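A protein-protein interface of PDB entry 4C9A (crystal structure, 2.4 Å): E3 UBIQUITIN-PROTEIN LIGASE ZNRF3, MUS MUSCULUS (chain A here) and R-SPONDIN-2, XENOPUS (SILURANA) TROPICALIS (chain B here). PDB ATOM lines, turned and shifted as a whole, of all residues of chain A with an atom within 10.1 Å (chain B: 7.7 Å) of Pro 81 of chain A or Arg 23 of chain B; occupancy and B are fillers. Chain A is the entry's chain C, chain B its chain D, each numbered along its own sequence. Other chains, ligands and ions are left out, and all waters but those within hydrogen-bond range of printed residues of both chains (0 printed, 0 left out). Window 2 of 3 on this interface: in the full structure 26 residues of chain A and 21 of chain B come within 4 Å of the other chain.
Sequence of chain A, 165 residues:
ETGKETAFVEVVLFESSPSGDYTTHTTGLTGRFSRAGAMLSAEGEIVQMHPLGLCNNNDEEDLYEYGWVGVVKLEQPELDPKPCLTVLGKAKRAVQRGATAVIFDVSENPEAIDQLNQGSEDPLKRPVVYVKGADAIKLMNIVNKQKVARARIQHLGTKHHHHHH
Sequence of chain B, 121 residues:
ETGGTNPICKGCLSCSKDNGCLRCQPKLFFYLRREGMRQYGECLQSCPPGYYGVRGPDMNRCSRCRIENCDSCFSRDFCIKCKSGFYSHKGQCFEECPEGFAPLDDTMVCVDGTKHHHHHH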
ATOM      1  N   HIS A  50     -18.866 -16.391 -22.679  1.00  0.00           N
ATOM      2  CA  HIS A  50     -18.985 -15.737 -21.389  1.00  0.00           C
ATOM      3  C   HIS A  50     -20.013 -16.603 -20.682  1.00  0.00           C
ATOM      4  O   HIS A  50     -20.924 -17.090 -21.320  1.00  0.00           O
ATOM      5  CB  HIS A  50     -19.449 -14.291 -21.571  1.00  0.00           C
ATOM      6  CG  HIS A  50     -19.459 -13.480 -20.314  1.00  0.00           C
ATOM      7  ND1 HIS A  50     -20.272 -13.766 -19.237  1.00  0.00           N
ATOM      8  CD2 HIS A  50     -18.786 -12.353 -19.980  1.00  0.00           C
ATOM      9  CE1 HIS A  50     -20.070 -12.879 -18.281  1.00  0.00           C
ATOM     10  NE2 HIS A  50     -19.161 -12.017 -18.706  1.00  0.00           N
ATOM     11  N   PRO A  51     -19.859 -16.810 -19.382  1.00  0.00           N
ATOM     12  CA  PRO A  51     -20.769 -17.576 -18.559  1.00  0.00           C
ATOM     13  C   PRO A  51     -22.216 -17.214 -18.749  1.00  0.00           C
ATOM     14  O   PRO A  51     -23.035 -18.089 -19.005  1.00  0.00           O
ATOM     15  CB  PRO A  51     -20.318 -17.218 -17.153  1.00  0.00           C
ATOM     16  CG  PRO A  51     -18.864 -17.061 -17.288  1.00  0.00           C
ATOM     17  CD  PRO A  51     -18.643 -16.449 -18.636  1.00  0.00           C
ATOM     18  N   LEU A  52     -22.536 -15.939 -18.597  1.00  0.00           N
ATOM     19  CA  LEU A  52     -23.857 -15.394 -19.007  1.00  0.00           C
ATOM     20  C   LEU A  52     -24.137 -15.491 -20.530  1.00  0.00           C
ATOM     21  O   LEU A  52     -25.224 -15.176 -20.973  1.00  0.00           O
ATOM     22  CB  LEU A  52     -23.972 -13.918 -18.584  1.00  0.00           C
ATOM     23  CG  LEU A  52     -24.209 -13.619 -17.103  1.00  0.00           C
ATOM     24  CD1 LEU A  52     -22.937 -13.289 -16.336  1.00  0.00           C
ATOM     25  CD2 LEU A  52     -25.219 -12.463 -16.984  1.00  0.00           C
ATOM     26  N   GLU A  75     -16.410 -18.342 -12.897  1.00  0.00           N
ATOM     27  CA  GLU A  75     -16.126 -17.422 -11.832  1.00  0.00           C
ATOM     28  C   GLU A  75     -16.607 -17.985 -10.493  1.00  0.00           C
ATOM     29  O   GLU A  75     -17.419 -18.940 -10.423  1.00  0.00           O
ATOM     30  CB  GLU A  75     -16.845 -16.088 -12.108  1.00  0.00           C
ATOM     31  CG  GLU A  75     -16.489 -15.434 -13.439  1.00  0.00           C
ATOM     32  CD  GLU A  75     -15.106 -14.814 -13.455  1.00  0.00           C
ATOM     33  OE1 GLU A  75     -14.517 -14.697 -12.344  1.00  0.00           O
ATOM     34  OE2 GLU A  75     -14.625 -14.434 -14.566  1.00  0.00           O
ATOM     35  N   GLN A  76     -16.103 -17.353  -9.435  1.00  0.00           N
ATOM     36  CA  GLN A  76     -16.472 -17.694  -8.089  1.00  0.00           C
ATOM     37  C   GLN A  76     -17.954 -17.616  -8.087  1.00  0.00           C
ATOM     38  O   GLN A  76     -18.525 -16.618  -8.525  1.00  0.00           O
ATOM     39  CB  GLN A  76     -15.876 -16.716  -7.085  1.00  0.00           C
ATOM     40  CG  GLN A  76     -14.387 -16.444  -7.357  1.00  0.00           C
ATOM     41  CD  GLN A  76     -13.624 -15.844  -6.186  1.00  0.00           C
ATOM     42  OE1 GLN A  76     -12.736 -15.008  -6.381  1.00  0.00           O
ATOM     43  NE2 GLN A  76     -13.943 -16.283  -4.968  1.00  0.00           N
ATOM     44  N   PRO A  77     -18.600 -18.683  -7.628  1.00  0.00           N
ATOM     45  CA  PRO A  77     -20.061 -18.771  -7.753  1.00  0.00           C
ATOM     46  C   PRO A  77     -20.883 -17.676  -7.069  1.00  0.00           C
ATOM     47  O   PRO A  77     -22.107 -17.670  -7.248  1.00  0.00           O
ATOM     48  CB  PRO A  77     -20.400 -20.153  -7.155  1.00  0.00           C
ATOM     49  CG  PRO A  77     -19.231 -20.536  -6.324  1.00  0.00           C
ATOM     50  CD  PRO A  77     -18.023 -19.813  -6.879  1.00  0.00           C
ATOM     51  N   GLU A  78     -20.252 -16.781  -6.295  1.00  0.00           N
ATOM     52  CA  GLU A  78     -20.991 -15.673  -5.634  1.00  0.00           C
ATOM     53  C   GLU A  78     -21.084 -14.446  -6.505  1.00  0.00           C
ATOM     54  O   GLU A  78     -21.890 -13.561  -6.239  1.00  0.00           O
ATOM     55  CB  GLU A  78     -20.384 -15.270  -4.297  1.00  0.00           C
ATOM     56  CG  GLU A  78     -20.363 -16.400  -3.288  1.00  0.00           C
ATOM     57  CD  GLU A  78     -19.119 -17.280  -3.384  1.00  0.00           C
ATOM     58  OE1 GLU A  78     -18.433 -17.307  -4.454  1.00  0.00           O
ATOM     59  OE2 GLU A  78     -18.827 -17.950  -2.365  1.00  0.00           O
ATOM     60  N   LEU A  79     -20.269 -14.392  -7.550  1.00  0.00           N
ATOM     61  CA  LEU A  79     -20.352 -13.294  -8.519  1.00  0.00           C
ATOM     62  C   LEU A  79     -21.659 -13.338  -9.353  1.00  0.00           C
ATOM     63  O   LEU A  79     -22.138 -12.304  -9.844  1.00  0.00           O
ATOM     64  CB  LEU A  79     -19.108 -13.305  -9.399  1.00  0.00           C
ATOM     65  CG  LEU A  79     -17.854 -13.061  -8.554  1.00  0.00           C
ATOM     66  CD1 LEU A  79     -16.640 -13.796  -9.110  1.00  0.00           C
ATOM     67  CD2 LEU A  79     -17.610 -11.563  -8.435  1.00  0.00           C
ATOM     68  N   ASP A  80     -22.228 -14.535  -9.508  1.00  0.00           N
ATOM     69  CA  ASP A  80     -23.635 -14.673  -9.896  1.00  0.00           C
ATOM     70  C   ASP A  80     -24.346 -15.598  -8.914  1.00  0.00           C
ATOM     71  O   ASP A  80     -24.294 -16.820  -9.067  1.00  0.00           O
ATOM     72  CB  ASP A  80     -23.793 -15.201 -11.320  1.00  0.00           C
ATOM     73  CG  ASP A  80     -25.172 -14.922 -11.878  1.00  0.00           C
ATOM     74  OD1 ASP A  80     -26.142 -14.860 -11.079  1.00  0.00           O
ATOM     75  OD2 ASP A  80     -25.276 -14.744 -13.110  1.00  0.00           O
ATOM     76  N   PRO A  81     -25.016 -15.018  -7.903  1.00  0.00           N
ATOM     77  CA  PRO A  81     -25.623 -15.861  -6.866  1.00  0.00           C
ATOM     78  C   PRO A  81     -26.775 -16.744  -7.394  1.00  0.00           C
ATOM     79  O   PRO A  81     -26.877 -17.933  -7.010  1.00  0.00           O
ATOM     80  CB  PRO A  81     -26.107 -14.848  -5.808  1.00  0.00           C
ATOM     81  CG  PRO A  81     -25.746 -13.479  -6.311  1.00  0.00           C
ATOM     82  CD  PRO A  81     -25.375 -13.593  -7.754  1.00  0.00           C
ATOM     83  N   LYS A  82     -27.598 -16.173  -8.278  1.00  0.00           N
ATOM     84  CA  LYS A  82     -28.706 -16.903  -8.900  1.00  0.00           C
ATOM     85  C   LYS A  82     -28.638 -16.981 -10.450  1.00  0.00           C
ATOM     86  O   LYS A  82     -29.277 -16.209 -11.164  1.00  0.00           O
ATOM     87  CB  LYS A  82     -30.037 -16.390  -8.331  1.00  0.00           C
ATOM     88  CG  LYS A  82     -30.415 -17.241  -7.113  1.00  0.00           C
ATOM     89  CD  LYS A  82     -30.859 -16.490  -5.860  1.00  0.00           C
ATOM     90  CE  LYS A  82     -31.124 -17.477  -4.714  1.00  0.00           C
ATOM     91  NZ  LYS A  82     -32.313 -17.111  -3.878  1.00  0.00           N
ATOM     92  N   PRO A  83     -27.849 -17.946 -10.958  1.00  0.00           N
ATOM     93  CA  PRO A  83     -27.548 -18.066 -12.386  1.00  0.00           C
ATOM     94  C   PRO A  83     -28.744 -18.395 -13.233  1.00  0.00           C
ATOM     95  O   PRO A  83     -29.645 -19.092 -12.771  1.00  0.00           O
ATOM     96  CB  PRO A  83     -26.600 -19.273 -12.437  1.00  0.00           C
ATOM     97  CG  PRO A  83     -26.963 -20.082 -11.234  1.00  0.00           C
ATOM     98  CD  PRO A  83     -27.240 -19.051 -10.186  1.00  0.00           C
ATOM     99  N   CYS A  84     -28.717 -17.953 -14.483  1.00  0.00           N
ATOM    100  CA  CYS A  84     -29.762 -18.302 -15.438  1.00  0.00           C
ATOM    101  C   CYS A  84     -29.937 -19.826 -15.599  1.00  0.00           C
ATOM    102  O   CYS A  84     -31.051 -20.269 -15.873  1.00  0.00           O
ATOM    103  CB  CYS A  84     -29.497 -17.653 -16.806  1.00  0.00           C
ATOM    104  SG  CYS A  84     -28.022 -18.281 -17.680  1.00  0.00           S
ATOM    105  N   LEU A  85     -28.855 -20.603 -15.440  1.00  0.00           N
ATOM    106  CA  LEU A  85     -28.846 -22.087 -15.600  1.00  0.00           C
ATOM    107  C   LEU A  85     -27.762 -22.705 -14.769  1.00  0.00           C
ATOM    108  O   LEU A  85     -26.867 -22.030 -14.300  1.00  0.00           O
ATOM    109  CB  LEU A  85     -28.449 -22.493 -17.018  1.00  0.00           C
ATOM    110  CG  LEU A  85     -29.257 -21.987 -18.232  1.00  0.00           C
ATOM    111  CD1 LEU A  85     -28.441 -22.048 -19.501  1.00  0.00           C
ATOM    112  CD2 LEU A  85     -30.524 -22.783 -18.403  1.00  0.00           C
ATOM    113  N   THR A  86     -27.771 -24.013 -14.652  1.00  0.00           N
ATOM    114  CA  THR A  86     -26.649 -24.657 -14.010  1.00  0.00           C
ATOM    115  C   THR A  86     -25.523 -24.739 -15.027  1.00  0.00           C
ATOM    116  O   THR A  86     -25.647 -24.260 -16.131  1.00  0.00           O
ATOM    117  CB  THR A  86     -27.037 -26.034 -13.473  1.00  0.00           C
ATOM    118  OG1 THR A  86     -27.331 -26.913 -14.557  1.00  0.00           O
ATOM    119  CG2 THR A  86     -28.281 -25.903 -12.605  1.00  0.00           C
ATOM    120  N   GLN A 115     -20.860 -30.671  -9.512  1.00  0.00           N
ATOM    121  CA  GLN A 115     -22.182 -30.354 -10.067  1.00  0.00           C
ATOM    122  C   GLN A 115     -22.324 -30.995 -11.432  1.00  0.00           C
ATOM    123  O   GLN A 115     -23.334 -31.602 -11.783  1.00  0.00           O
ATOM    124  CB  GLN A 115     -22.405 -28.840 -10.183  1.00  0.00           C
ATOM    125  CG  GLN A 115     -22.422 -28.076  -8.859  1.00  0.00           C
ATOM    126  CD  GLN A 115     -22.059 -26.578  -8.985  1.00  0.00           C
ATOM    127  OE1 GLN A 115     -22.007 -25.984 -10.080  1.00  0.00           O
ATOM    128  NE2 GLN A 115     -21.820 -25.956  -7.845  1.00  0.00           N
ATOM    129  N   LYS B  10     -14.781  -1.150 -17.492  1.00  0.00           N
ATOM    130  CA  LYS B  10     -15.547  -0.174 -16.721  1.00  0.00           C
ATOM    131  C   LYS B  10     -17.061  -0.258 -16.884  1.00  0.00           C
ATOM    132  O   LYS B  10     -17.553  -0.786 -17.867  1.00  0.00           O
ATOM    133  CB  LYS B  10     -15.147   1.214 -17.182  1.00  0.00           C
ATOM    134  CG  LYS B  10     -15.806   1.628 -18.479  1.00  0.00           C
ATOM    135  CD  LYS B  10     -14.980   2.712 -19.153  1.00  0.00           C
ATOM    136  CE  LYS B  10     -15.678   3.275 -20.381  1.00  0.00           C
ATOM    137  NZ  LYS B  10     -15.337   4.707 -20.615  1.00  0.00           N
ATOM    138  N   GLY B  11     -17.772   0.373 -15.950  1.00  0.00           N
ATOM    139  CA  GLY B  11     -19.242   0.376 -15.863  1.00  0.00           C
ATOM    140  C   GLY B  11     -19.675  -0.762 -14.971  1.00  0.00           C
ATOM    141  O   GLY B  11     -20.843  -1.162 -14.883  1.00  0.00           O
ATOM    142  N   CYS B  12     -18.699  -1.231 -14.240  1.00  0.00           N
ATOM    143  CA  CYS B  12     -18.614  -2.591 -13.886  1.00  0.00           C
ATOM    144  C   CYS B  12     -18.764  -2.713 -12.408  1.00  0.00           C
ATOM    145  O   CYS B  12     -18.087  -2.008 -11.660  1.00  0.00           O
ATOM    146  CB  CYS B  12     -17.218  -3.013 -14.270  1.00  0.00           C
ATOM    147  SG  CYS B  12     -17.199  -4.597 -15.045  1.00  0.00           S
ATOM    148  N   LEU B  13     -19.630  -3.613 -11.975  1.00  0.00           N
ATOM    149  CA  LEU B  13     -19.662  -3.983 -10.569  1.00  0.00           C
ATOM    150  C   LEU B  13     -18.558  -5.017 -10.290  1.00  0.00           C
ATOM    151  O   LEU B  13     -17.628  -4.720  -9.555  1.00  0.00           O
ATOM    152  CB  LEU B  13     -21.056  -4.480 -10.147  1.00  0.00           C
ATOM    153  CG  LEU B  13     -22.187  -3.427 -10.091  1.00  0.00           C
ATOM    154  CD1 LEU B  13     -23.502  -4.044  -9.595  1.00  0.00           C
ATOM    155  CD2 LEU B  13     -21.788  -2.203  -9.256  1.00  0.00           C
ATOM    156  N   SER B  14     -18.652  -6.212 -10.880  1.00  0.00           N
ATOM    157  CA  SER B  14     -17.563  -7.210 -10.813  1.00  0.00           C
ATOM    158  C   SER B  14     -16.942  -7.286 -12.196  1.00  0.00           C
ATOM    159  O   SER B  14     -17.601  -6.948 -13.166  1.00  0.00           O
ATOM    160  CB  SER B  14     -18.057  -8.599 -10.397  1.00  0.00           C
ATOM    161  OG  SER B  14     -19.432  -8.610 -10.045  1.00  0.00           O
ATOM    162  N   CYS B  15     -15.695  -7.744 -12.273  1.00  0.00           N
ATOM    163  CA  CYS B  15     -14.852  -7.610 -13.479  1.00  0.00           C
ATOM    164  C   CYS B  15     -13.679  -8.643 -13.412  1.00  0.00           C
ATOM    165  O   CYS B  15     -13.043  -8.862 -12.335  1.00  0.00           O
ATOM    166  CB  CYS B  15     -14.411  -6.133 -13.620  1.00  0.00           C
ATOM    167  SG  CYS B  15     -12.909  -5.641 -14.518  1.00  0.00           S
ATOM    168  N   GLY B  20     -14.169 -10.024 -18.636  1.00  0.00           N
ATOM    169  CA  GLY B  20     -14.509  -8.611 -18.659  1.00  0.00           C
ATOM    170  C   GLY B  20     -15.610  -8.405 -17.643  1.00  0.00           C
ATOM    171  O   GLY B  20     -15.632  -9.097 -16.595  1.00  0.00           O
ATOM    172  N   CYS B  21     -16.541  -7.489 -17.944  1.00  0.00           N
ATOM    173  CA  CYS B  21     -17.567  -7.129 -16.962  1.00  0.00           C
ATOM    174  C   CYS B  21     -18.473  -8.334 -16.687  1.00  0.00           C
ATOM    175  O   CYS B  21     -18.876  -9.014 -17.624  1.00  0.00           O
ATOM    176  CB  CYS B  21     -18.379  -5.886 -17.428  1.00  0.00           C
ATOM    177  SG  CYS B  21     -17.600  -4.292 -17.038  1.00  0.00           S
ATOM    178  N   LEU B  22     -18.774  -8.603 -15.419  1.00  0.00           N
ATOM    179  CA  LEU B  22     -19.678  -9.715 -15.010  1.00  0.00           C
ATOM    180  C   LEU B  22     -21.066  -9.245 -14.530  1.00  0.00           C
ATOM    181  O   LEU B  22     -22.053  -9.999 -14.576  1.00  0.00           O
ATOM    182  CB  LEU B  22     -19.039 -10.547 -13.893  1.00  0.00           C
ATOM    183  CG  LEU B  22     -17.680 -11.148 -14.254  1.00  0.00           C
ATOM    184  CD1 LEU B  22     -16.824 -11.394 -13.022  1.00  0.00           C
ATOM    185  CD2 LEU B  22     -17.887 -12.434 -15.018  1.00  0.00           C
ATOM    186  N   ARG B  23     -21.132  -8.014 -14.045  1.00  0.00           N
ATOM    187  CA  ARG B  23     -22.395  -7.397 -13.682  1.00  0.00           C
ATOM    188  C   ARG B  23     -22.160  -5.941 -13.787  1.00  0.00           C
ATOM    189  O   ARG B  23     -21.059  -5.459 -13.587  1.00  0.00           O
ATOM    190  CB  ARG B  23     -22.868  -7.783 -12.262  1.00  0.00           C
ATOM    191  CG  ARG B  23     -23.708  -9.062 -12.260  1.00  0.00           C
ATOM    192  CD  ARG B  23     -23.838  -9.742 -10.893  1.00  0.00           C
ATOM    193  NE  ARG B  23     -24.985  -9.257 -10.112  1.00  0.00           N
ATOM    194  CZ  ARG B  23     -26.018  -9.997  -9.676  1.00  0.00           C
ATOM    195  NH1 ARG B  23     -26.107 -11.309  -9.910  1.00  0.00           N
ATOM    196  NH2 ARG B  23     -26.988  -9.409  -8.980  1.00  0.00           N
ATOM    197  N   CYS B  24     -23.216  -5.234 -14.102  1.00  0.00           N
ATOM    198  CA  CYS B  24     -23.122  -3.841 -14.378  1.00  0.00           C
ATOM    199  C   CYS B  24     -23.667  -2.992 -13.255  1.00  0.00           C
ATOM    200  O   CYS B  24     -24.607  -3.372 -12.576  1.00  0.00           O
ATOM    201  CB  CYS B  24     -23.915  -3.589 -15.636  1.00  0.00           C
ATOM    202  SG  CYS B  24     -23.145  -4.351 -17.088  1.00  0.00           S
ATOM    203  N   GLN B  25     -23.065  -1.825 -13.069  1.00  0.00           N
ATOM    204  CA  GLN B  25     -23.684  -0.764 -12.294  1.00  0.00           C
ATOM    205  C   GLN B  25     -25.137  -0.618 -12.747  1.00  0.00           C
ATOM    206  O   GLN B  25     -25.421  -0.633 -13.944  1.00  0.00           O
ATOM    207  CB  GLN B  25     -22.938   0.546 -12.478  1.00  0.00           C
ATOM    208  CG  GLN B  25     -21.629   0.627 -11.707  1.00  0.00           C
ATOM    209  CD  GLN B  25     -20.660   1.660 -12.303  1.00  0.00           C
ATOM    210  OE1 GLN B  25     -20.982   2.365 -13.276  1.00  0.00           O
ATOM    211  NE2 GLN B  25     -19.460   1.747 -11.723  1.00  0.00           N
ATOM    212  N   PRO B  26     -26.054  -0.473 -11.794  1.00  0.00           N
ATOM    213  CA  PRO B  26     -27.483  -0.770 -12.023  1.00  0.00           C
ATOM    214  C   PRO B  26     -28.234  -0.057 -13.150  1.00  0.00           C
ATOM    215  O   PRO B  26     -29.277  -0.594 -13.581  1.00  0.00           O
ATOM    216  CB  PRO B  26     -28.137  -0.418 -10.687  1.00  0.00           C
ATOM    217  CG  PRO B  26     -27.036  -0.592  -9.697  1.00  0.00           C
ATOM    218  CD  PRO B  26     -25.760  -0.224 -10.377  1.00  0.00           C
ATOM    219  N   LEU B  28     -26.907   0.670 -16.134  1.00  0.00           N
ATOM    220  CA  LEU B  28     -26.172   0.452 -17.389  1.00  0.00           C
ATOM    221  C   LEU B  28     -26.488  -0.896 -17.978  1.00  0.00           C
ATOM    222  O   LEU B  28     -26.887  -1.799 -17.250  1.00  0.00           O
ATOM    223  CB  LEU B  28     -24.665   0.483 -17.160  1.00  0.00           C
ATOM    224  CG  LEU B  28     -24.061   1.756 -16.635  1.00  0.00           C
ATOM    225  CD1 LEU B  28     -22.581   1.519 -16.509  1.00  0.00           C
ATOM    226  CD2 LEU B  28     -24.358   2.908 -17.584  1.00  0.00           C
ATOM    227  N   PHE B  30     -25.742  -4.437 -19.886  1.00  0.00           N
ATOM    228  CA  PHE B  30     -24.776  -5.529 -20.108  1.00  0.00           C
ATOM    229  C   PHE B  30     -24.692  -6.006 -21.566  1.00  0.00           C
ATOM    230  O   PHE B  30     -25.693  -6.401 -22.136  1.00  0.00           O
ATOM    231  CB  PHE B  30     -25.125  -6.706 -19.245  1.00  0.00           C
ATOM    232  CG  PHE B  30     -24.143  -7.814 -19.336  1.00  0.00           C
ATOM    233  CD1 PHE B  30     -22.873  -7.668 -18.793  1.00  0.00           C
ATOM    234  CD2 PHE B  30     -24.478  -9.007 -19.968  1.00  0.00           C
ATOM    235  CE1 PHE B  30     -21.969  -8.708 -18.853  1.00  0.00           C
ATOM    236  CE2 PHE B  30     -23.563 -10.039 -20.051  1.00  0.00           C
ATOM    237  CZ  PHE B  30     -22.321  -9.902 -19.478  1.00  0.00           C
ATOM    238  N   GLY B  41     -17.876  -9.321 -21.226  1.00  0.00           N
ATOM    239  CA  GLY B  41     -18.925  -8.349 -20.933  1.00  0.00           C
ATOM    240  C   GLY B  41     -18.434  -6.924 -20.973  1.00  0.00           C
ATOM    241  O   GLY B  41     -17.354  -6.619 -20.472  1.00  0.00           O
ATOM    242  N   GLU B  42     -19.243  -6.062 -21.574  1.00  0.00           N
ATOM    243  CA  GLU B  42     -19.132  -4.618 -21.408  1.00  0.00           C
ATOM    244  C   GLU B  42     -20.413  -4.162 -20.738  1.00  0.00           C
ATOM    245  O   GLU B  42     -21.475  -4.763 -20.914  1.00  0.00           O
ATOM    246  CB  GLU B  42     -18.990  -3.879 -22.745  1.00  0.00           C
ATOM    247  CG  GLU B  42     -18.067  -4.494 -23.784  1.00  0.00           C
ATOM    248  CD  GLU B  42     -17.801  -3.519 -24.949  1.00  0.00           C
ATOM    249  OE1 GLU B  42     -18.596  -3.338 -25.944  1.00  0.00           O
ATOM    250  OE2 GLU B  42     -16.744  -2.908 -24.851  1.00  0.00           O
ATOM    251  N   CYS B  43     -20.301  -3.086 -19.980  1.00  0.00           N
ATOM    252  CA  CYS B  43     -21.430  -2.427 -19.333  1.00  0.00           C
ATOM    253  C   CYS B  43     -21.530  -1.080 -19.997  1.00  0.00           C
ATOM    254  O   CYS B  43     -20.633  -0.271 -19.832  1.00  0.00           O
ATOM    255  CB  CYS B  43     -21.151  -2.255 -17.842  1.00  0.00           C
ATOM    256  SG  CYS B  43     -21.198  -3.810 -16.917  1.00  0.00           S
ATOM    257  N   PRO B  57     -35.441  -6.091 -13.584  1.00  0.00           N
ATOM    258  CA  PRO B  57     -35.020  -6.021 -12.182  1.00  0.00           C
ATOM    259  C   PRO B  57     -33.654  -6.657 -12.004  1.00  0.00           C
ATOM    260  O   PRO B  57     -32.821  -6.097 -11.308  1.00  0.00           O
ATOM    261  CB  PRO B  57     -36.099  -6.823 -11.432  1.00  0.00           C
ATOM    262  CG  PRO B  57     -36.691  -7.744 -12.456  1.00  0.00           C
ATOM    263  CD  PRO B  57     -36.579  -7.024 -13.778  1.00  0.00           C
ATOM    264  N   ASP B  58     -33.423  -7.800 -12.657  1.00  0.00           N
ATOM    265  CA  ASP B  58     -32.159  -8.540 -12.513  1.00  0.00           C
ATOM    266  C   ASP B  58     -31.004  -7.759 -13.143  1.00  0.00           C
ATOM    267  O   ASP B  58     -29.943  -7.627 -12.547  1.00  0.00           O
ATOM    268  CB  ASP B  58     -32.211  -9.941 -13.164  1.00  0.00           C
ATOM    269  CG  ASP B  58     -33.638 -10.455 -13.411  1.00  0.00           C
ATOM    270  OD1 ASP B  58     -34.585 -10.001 -12.722  1.00  0.00           O
ATOM    271  OD2 ASP B  58     -33.792 -11.341 -14.300  1.00  0.00           O
ATOM    272  N   MET B  59     -31.208  -7.267 -14.363  1.00  0.00           N
ATOM    273  CA  MET B  59     -30.213  -6.445 -15.062  1.00  0.00           C
ATOM    274  C   MET B  59     -30.780  -5.991 -16.373  1.00  0.00           C
ATOM    275  O   MET B  59     -31.852  -6.410 -16.760  1.00  0.00           O
ATOM    276  CB  MET B  59     -28.884  -7.168 -15.343  1.00  0.00           C
ATOM    277  CG  MET B  59     -28.957  -8.305 -16.378  1.00  0.00           C
ATOM    278  SD  MET B  59     -27.203  -9.226 -16.596  1.00  0.00           S
ATOM    279  CE  MET B  59     -25.981  -8.052 -15.569  1.00  0.00           C
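NE2 of His 50 of chain A sits at hydrogen-bond distance from O of Cys 21 of chain B, at 3.2 Å. NH1 of Arg 23 of chain B lies within salt-bridge range of OD1 of Asp 80 of chain A, at 3.7 Å.
The backbone NH of Cys 21 of chain B lies within hydrogen-bond range of the backbone carbonyl oxygen of Gly 41 of chain B (2.8 Å). ND1 of His 50 of chain A is in hydrogen-bond range of N of Leu 52 of chain A, at 3.2 Å. The backbone NH (N) of Leu 22 of chain B is in hydrogen-bond range of the backbone carbonyl oxygen (O) of Ser 14 of chain B (3.0 Å). The side-chain sulfur of Cys 21 of chain B is disulfide-bonded to the side-chain sulfur of Cys 12 of chain B, 2.1 Å away. N of Leu 13 of chain B sits at hydrogen-bond distance from O of Arg 23 of chain B, 2.8 Å away. The side-chain carboxylate of Asp 80 of chain A lies close to the backbone NH of Lys 82 of chain A.
Leu 22 of chain B touches His 50 of chain A. His 50 of chain A touches Phe 30 of chain B. N of Gly 41 of chain B touches CD2 of His 50 of chain A, at 3.4 Å. CD1 of Leu 52 of chain A touches O of Leu 22 of chain B, 3.8 Å away. Leu 52 of chain A touches Met 59 of chain B. Glu 75 of chain A touches Leu 22 of chain B (CG to CD2, 3.7 Å). CD2 of Leu 79 of chain A touches CB of Ser 14 of chain B, at 3.6 Å. Arg 23 of chain B touches Leu 79 of chain A. NH1 of Arg 23 of chain B touches CD of Pro 81 of chain A, at 3.2 Å.
Of the printed residues of chain B, His 50 of chain A touches Cys 21, Leu 22, Phe 30 and Gly 41. Of the printed residues of chain B, Glu 75 of chain A touches Leu 22 (3.7 Å). Of the printed residues of chain B, Leu 79 of chain A touches Ser 14 and Arg 23. Pro 81 of chain A touches just one residue of chain B: Arg 23. No residue of chain A comes within 4 Å of Cys 12 of chain B. Ser 14 of chain B touches just one residue of chain A: Leu 79. Leu 22 of chain B touches three residues of chain A. Arg 23 of chain B touches just these residues of chain A: Leu 79 (3.2 Å), Asp 80 (3.7 Å) and Pro 81 (3.2 Å). Gln 25 of chain B touches none of the printed residues of chain A. Printed residues of chain A within 4 Å of Phe 30 of chain B: His 50 (3.9 Å). Printed residues of chain A within 4 Å of Met 59 of chain B: Leu 52. The nearest printed residue of chain B that does not touch Pro 81 of chain A is Ser 14 of chain B (8.1 Å). The nearest residue of chain A that does not touch Arg 23 of chain B is Lys 82 of chain A (5.3 Å).
Of the 21 printed residues of chain B, 7 touch a printed residue of chain A. Hydrophobic or aromatic side chains of chain B that line the printed part of chain A: Leu 22, Phe 30 and Met 59. Hydrophobic or aromatic side chains of chain A that line the printed part of chain B: His 50, Leu 52, Leu 79 and Pro 81.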
